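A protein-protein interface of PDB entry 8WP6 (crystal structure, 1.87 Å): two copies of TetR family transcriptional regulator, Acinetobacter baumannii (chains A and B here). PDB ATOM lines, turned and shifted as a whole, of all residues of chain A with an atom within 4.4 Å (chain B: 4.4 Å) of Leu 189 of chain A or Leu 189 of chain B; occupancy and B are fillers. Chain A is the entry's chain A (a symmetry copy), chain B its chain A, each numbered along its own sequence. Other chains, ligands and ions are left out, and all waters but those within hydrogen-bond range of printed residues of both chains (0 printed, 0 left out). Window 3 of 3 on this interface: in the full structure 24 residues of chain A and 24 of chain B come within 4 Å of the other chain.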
ATOM      1  N   ARG A 146     -23.724   4.905 -16.179  1.00  0.00           N
ATOM      2  CA  ARG A 146     -24.631   5.921 -15.653  1.00  0.00           C
ATOM      3  C   ARG A 146     -23.887   7.189 -15.250  1.00  0.00           C
ATOM      4  O   ARG A 146     -24.444   8.288 -15.345  1.00  0.00           O
ATOM      5  CB  ARG A 146     -25.421   5.371 -14.464  1.00  0.00           C
ATOM      6  CG  ARG A 146     -24.634   4.447 -13.556  1.00  0.00           C
ATOM      7  CD  ARG A 146     -25.540   3.759 -12.546  1.00  0.00           C
ATOM      8  NE  ARG A 146     -26.394   2.753 -13.169  1.00  0.00           N
ATOM      9  CZ  ARG A 146     -26.250   1.445 -13.005  1.00  0.00           C
ATOM     10  NH1 ARG A 146     -25.276   0.944 -12.263  1.00  0.00           N
ATOM     11  NH2 ARG A 146     -27.103   0.620 -13.604  1.00  0.00           N
ATOM     12  N   ALA A 185     -20.528  -4.504  -2.910  1.00  0.00           N
ATOM     13  CA  ALA A 185     -21.817  -3.828  -2.995  1.00  0.00           C
ATOM     14  C   ALA A 185     -21.693  -2.482  -3.695  1.00  0.00           C
ATOM     15  O   ALA A 185     -22.540  -2.127  -4.523  1.00  0.00           O
ATOM     16  CB  ALA A 185     -22.409  -3.652  -1.596  1.00  0.00           C
ATOM     17  N   ILE A 186     -20.644  -1.722  -3.380  1.00  0.00           N
ATOM     18  CA  ILE A 186     -20.479  -0.405  -3.986  1.00  0.00           C
ATOM     19  C   ILE A 186     -20.146  -0.533  -5.466  1.00  0.00           C
ATOM     20  O   ILE A 186     -20.704   0.186  -6.303  1.00  0.00           O
ATOM     21  CB  ILE A 186     -19.412   0.404  -3.226  1.00  0.00           C
ATOM     22  CG1 ILE A 186     -19.926   0.778  -1.836  1.00  0.00           C
ATOM     23  CG2 ILE A 186     -19.044   1.665  -3.993  1.00  0.00           C
ATOM     24  CD1 ILE A 186     -21.114   1.726  -1.862  1.00  0.00           C
ATOM     25  N   ILE A 187     -19.233  -1.447  -5.815  1.00  0.00           N
ATOM     26  CA  ILE A 187     -18.908  -1.681  -7.223  1.00  0.00           C
ATOM     27  C   ILE A 187     -20.168  -2.024  -8.007  1.00  0.00           C
ATOM     28  O   ILE A 187     -20.419  -1.478  -9.088  1.00  0.00           O
ATOM     29  CB  ILE A 187     -17.843  -2.785  -7.357  1.00  0.00           C
ATOM     30  CG1 ILE A 187     -16.499  -2.312  -6.807  1.00  0.00           C
ATOM     31  CG2 ILE A 187     -17.662  -3.178  -8.817  1.00  0.00           C
ATOM     32  CD1 ILE A 187     -15.469  -3.424  -6.700  1.00  0.00           C
ATOM     33  N   ARG A 188     -20.989  -2.924  -7.459  1.00  0.00           N
ATOM     34  CA  ARG A 188     -22.227  -3.318  -8.129  1.00  0.00           C
ATOM     35  C   ARG A 188     -23.163  -2.133  -8.328  1.00  0.00           C
ATOM     36  O   ARG A 188     -23.766  -1.986  -9.396  1.00  0.00           O
ATOM     37  CB  ARG A 188     -22.927  -4.416  -7.332  1.00  0.00           C
ATOM     38  CG  ARG A 188     -22.265  -5.771  -7.441  1.00  0.00           C
ATOM     39  CD  ARG A 188     -23.135  -6.861  -6.835  1.00  0.00           C
ATOM     40  NE  ARG A 188     -22.513  -8.170  -6.979  1.00  0.00           N
ATOM     41  CZ  ARG A 188     -22.655  -8.945  -8.046  1.00  0.00           C
ATOM     42  NH1 ARG A 188     -23.416  -8.582  -9.065  1.00  0.00           N
ATOM     43  NH2 ARG A 188     -22.018 -10.111  -8.091  1.00  0.00           N
ATOM     44  N   LEU A 189     -23.308  -1.279  -7.312  1.00  0.00           N
ATOM     45  CA  LEU A 189     -24.234  -0.157  -7.436  1.00  0.00           C
ATOM     46  C   LEU A 189     -23.753   0.840  -8.480  1.00  0.00           C
ATOM     47  O   LEU A 189     -24.562   1.427  -9.208  1.00  0.00           O
ATOM     48  CB  LEU A 189     -24.417   0.537  -6.085  1.00  0.00           C
ATOM     49  CG  LEU A 189     -25.069  -0.291  -4.978  1.00  0.00           C
ATOM     50  CD1 LEU A 189     -25.021   0.468  -3.659  1.00  0.00           C
ATOM     51  CD2 LEU A 189     -26.499  -0.671  -5.346  1.00  0.00           C
ATOM     52  N   GLU A 190     -22.440   1.046  -8.570  1.00  0.00           N
ATOM     53  CA  GLU A 190     -21.915   2.058  -9.476  1.00  0.00           C
ATOM     54  C   GLU A 190     -21.874   1.572 -10.919  1.00  0.00           C
ATOM     55  O   GLU A 190     -22.077   2.369 -11.841  1.00  0.00           O
ATOM     56  CB  GLU A 190     -20.509   2.479  -9.035  1.00  0.00           C
ATOM     57  CG  GLU A 190     -20.480   3.341  -7.778  1.00  0.00           C
ATOM     58  CD  GLU A 190     -20.467   4.832  -8.074  1.00  0.00           C
ATOM     59  OE1 GLU A 190     -20.958   5.240  -9.149  1.00  0.00           O
ATOM     60  OE2 GLU A 190     -19.965   5.598  -7.225  1.00  0.00           O
ATOM     61  N   LEU A 191     -21.589   0.302 -11.109  1.00  0.00           N
ATOM     62  CA  LEU A 191     -21.343  -0.205 -12.449  1.00  0.00           C
ATOM     63  C   LEU A 191     -22.087  -1.420 -12.950  1.00  0.00           C
ATOM     64  O   LEU A 191     -22.091  -1.660 -14.126  1.00  0.00           O
ATOM     65  CB  LEU A 191     -19.865  -0.560 -12.516  1.00  0.00           C
ATOM     66  CG  LEU A 191     -18.840   0.538 -12.340  1.00  0.00           C
ATOM     67  CD1 LEU A 191     -17.577  -0.061 -11.791  1.00  0.00           C
ATOM     68  CD2 LEU A 191     -18.578   1.198 -13.664  1.00  0.00           C
ATOM     69  N   ARG B 146     -32.734  -2.634  -0.364  1.00  0.00           N
ATOM     70  CA  ARG B 146     -31.935  -3.694  -0.973  1.00  0.00           C
ATOM     71  C   ARG B 146     -30.887  -4.235  -0.008  1.00  0.00           C
ATOM     72  O   ARG B 146     -30.541  -5.420  -0.074  1.00  0.00           O
ATOM     73  CB  ARG B 146     -31.267  -3.192  -2.254  1.00  0.00           C
ATOM     74  CG  ARG B 146     -30.787  -1.756  -2.196  1.00  0.00           C
ATOM     75  CD  ARG B 146     -30.356  -1.260  -3.568  1.00  0.00           C
ATOM     76  NE  ARG B 146     -31.491  -1.060  -4.463  1.00  0.00           N
ATOM     77  CZ  ARG B 146     -31.934   0.127  -4.854  1.00  0.00           C
ATOM     78  NH1 ARG B 146     -31.376   1.249  -4.429  1.00  0.00           N
ATOM     79  NH2 ARG B 146     -32.964   0.190  -5.693  1.00  0.00           N
ATOM     80  N   ALA B 185     -25.041  11.187  -5.326  1.00  0.00           N
ATOM     81  CA  ALA B 185     -24.989  10.010  -6.184  1.00  0.00           C
ATOM     82  C   ALA B 185     -24.958   8.726  -5.367  1.00  0.00           C
ATOM     83  O   ALA B 185     -25.640   7.752  -5.705  1.00  0.00           O
ATOM     84  CB  ALA B 185     -23.771  10.087  -7.107  1.00  0.00           C
ATOM     85  N   ILE B 186     -24.178   8.708  -4.285  1.00  0.00           N
ATOM     86  CA  ILE B 186     -24.073   7.499  -3.474  1.00  0.00           C
ATOM     87  C   ILE B 186     -25.377   7.235  -2.734  1.00  0.00           C
ATOM     88  O   ILE B 186     -25.855   6.096  -2.688  1.00  0.00           O
ATOM     89  CB  ILE B 186     -22.878   7.607  -2.508  1.00  0.00           C
ATOM     90  CG1 ILE B 186     -21.564   7.557  -3.288  1.00  0.00           C
ATOM     91  CG2 ILE B 186     -22.909   6.482  -1.485  1.00  0.00           C
ATOM     92  CD1 ILE B 186     -21.319   6.227  -3.982  1.00  0.00           C
ATOM     93  N   ILE B 187     -25.973   8.277  -2.144  1.00  0.00           N
ATOM     94  CA  ILE B 187     -27.264   8.119  -1.473  1.00  0.00           C
ATOM     95  C   ILE B 187     -28.292   7.535  -2.434  1.00  0.00           C
ATOM     96  O   ILE B 187     -29.019   6.593  -2.100  1.00  0.00           O
ATOM     97  CB  ILE B 187     -27.739   9.462  -0.889  1.00  0.00           C
ATOM     98  CG1 ILE B 187     -26.843   9.897   0.269  1.00  0.00           C
ATOM     99  CG2 ILE B 187     -29.171   9.349  -0.383  1.00  0.00           C
ATOM    100  CD1 ILE B 187     -27.117  11.316   0.740  1.00  0.00           C
ATOM    101  N   ARG B 188     -28.350   8.079  -3.653  1.00  0.00           N
ATOM    102  CA  ARG B 188     -29.298   7.587  -4.650  1.00  0.00           C
ATOM    103  C   ARG B 188     -29.058   6.121  -4.983  1.00  0.00           C
ATOM    104  O   ARG B 188     -30.011   5.344  -5.101  1.00  0.00           O
ATOM    105  CB  ARG B 188     -29.214   8.437  -5.917  1.00  0.00           C
ATOM    106  CG  ARG B 188     -29.841   9.806  -5.782  1.00  0.00           C
ATOM    107  CD  ARG B 188     -29.944  10.501  -7.130  1.00  0.00           C
ATOM    108  NE  ARG B 188     -30.586  11.802  -7.001  1.00  0.00           N
ATOM    109  CZ  ARG B 188     -31.899  11.988  -7.044  1.00  0.00           C
ATOM    110  NH1 ARG B 188     -32.731  10.979  -7.241  1.00  0.00           N
ATOM    111  NH2 ARG B 188     -32.387  13.214  -6.885  1.00  0.00           N
ATOM    112  N   LEU B 189     -27.796   5.720  -5.146  1.00  0.00           N
ATOM    113  CA  LEU B 189     -27.518   4.335  -5.516  1.00  0.00           C
ATOM    114  C   LEU B 189     -27.898   3.379  -4.395  1.00  0.00           C
ATOM    115  O   LEU B 189     -28.379   2.269  -4.652  1.00  0.00           O
ATOM    116  CB  LEU B 189     -26.042   4.164  -5.881  1.00  0.00           C
ATOM    117  CG  LEU B 189     -25.553   4.926  -7.113  1.00  0.00           C
ATOM    118  CD1 LEU B 189     -24.042   4.800  -7.242  1.00  0.00           C
ATOM    119  CD2 LEU B 189     -26.260   4.442  -8.375  1.00  0.00           C
ATOM    120  N   GLU B 190     -27.690   3.790  -3.145  1.00  0.00           N
ATOM    121  CA  GLU B 190     -27.935   2.890  -2.025  1.00  0.00           C
ATOM    122  C   GLU B 190     -29.416   2.793  -1.681  1.00  0.00           C
ATOM    123  O   GLU B 190     -29.881   1.725  -1.269  1.00  0.00           O
ATOM    124  CB  GLU B 190     -27.150   3.357  -0.795  1.00  0.00           C
ATOM    125  CG  GLU B 190     -25.648   3.115  -0.884  1.00  0.00           C
ATOM    126  CD  GLU B 190     -25.213   1.806  -0.246  1.00  0.00           C
ATOM    127  OE1 GLU B 190     -26.034   0.866  -0.172  1.00  0.00           O
ATOM    128  OE2 GLU B 190     -24.042   1.717   0.181  1.00  0.00           O
ATOM    129  N   LEU B 191     -30.130   3.889  -1.818  1.00  0.00           N
ATOM    130  CA  LEU B 191     -31.500   3.940  -1.336  1.00  0.00           C
ATOM    131  C   LEU B 191     -32.610   4.404  -2.249  1.00  0.00           C
ATOM    132  O   LEU B 191     -33.749   4.182  -1.946  1.00  0.00           O
ATOM    133  CB  LEU B 191     -31.508   4.891  -0.148  1.00  0.00           C
ATOM    134  CG  LEU B 191     -30.696   4.538   1.078  1.00  0.00           C
ATOM    135  CD1 LEU B 191     -30.311   5.804   1.786  1.00  0.00           C
ATOM    136  CD2 LEU B 191     -31.509   3.654   1.981  1.00  0.00           C
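The backbone carbonyl oxygen (O) of Leu 189 of chain B sits at hydrogen-bond distance from the guanidinium group (NH1) of Arg 146 of chain B (3.2 Å).
The backbone carbonyl oxygen (O) of Leu 189 of chain A sits at hydrogen-bond distance from the guanidinium group (NH1) of Arg 146 of chain A.
Among the printed residues, pairs that only touch across the chains: Leu 189 of chain A with Leu 189 of chain B, Glu 190 of chain A with Ile 186 of chain B, Ile 186 of chain A with Glu 190 of chain B, Glu 190 of chain A with Leu 189 of chain B and Leu 189 of chain A with Glu 190 of chain B.
Of the printed residues of chain B, Ile 186 of chain A touches Glu 190.
Leu 189 of chain A touches just these residues of chain B: Leu 189 and Glu 190.
Of the printed residues of chain A, Ile 186 of chain B touches Glu 190 (3.6 Å).
Of chain A, only Leu 189 and Glu 190 come within 4 Å of Leu 189 of chain B.
Of the printed residues of chain A, Glu 190 of chain B touches Ile 186 and Leu 189.
The nearest residue of chain A that does not touch Leu 189 of chain B is Arg 146 of chain A (4.3 Å).
Of the 8 printed residues of chain A, 3 touch a printed residue of chain B.
Hydrophobic or aromatic side chains of chain A within 4 Å of the printed part of chain B: Ile 186 and Leu 189.
Printed residues of chain B that touch a printed residue of chain A: Ile 186, Leu 189 and Glu 190.
Hydrophobic or aromatic side chains of chain B that line the printed part of chain A: Ile 186 and Leu 189.
Among the printed residues, no Asp or Glu carboxylate lies within 4 Å of a Lys or Arg side-chain nitrogen of the other chain.
Ile 186 of chain A touches Glu 190 of chain B, and with the chains exchanged Glu 190 of chain A touches Ile 186 of chain B.
Leu 189 of chain B touches its own counterpart, Leu 189 of chain A.
Leu 189 of chain A touches Glu 190 of chain B, and with the chains exchanged Glu 190 of chain A touches Leu 189 of chain B.
Positions printed for both chains: 146, 185, 186, 187, 188, 189, 190 and 191.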
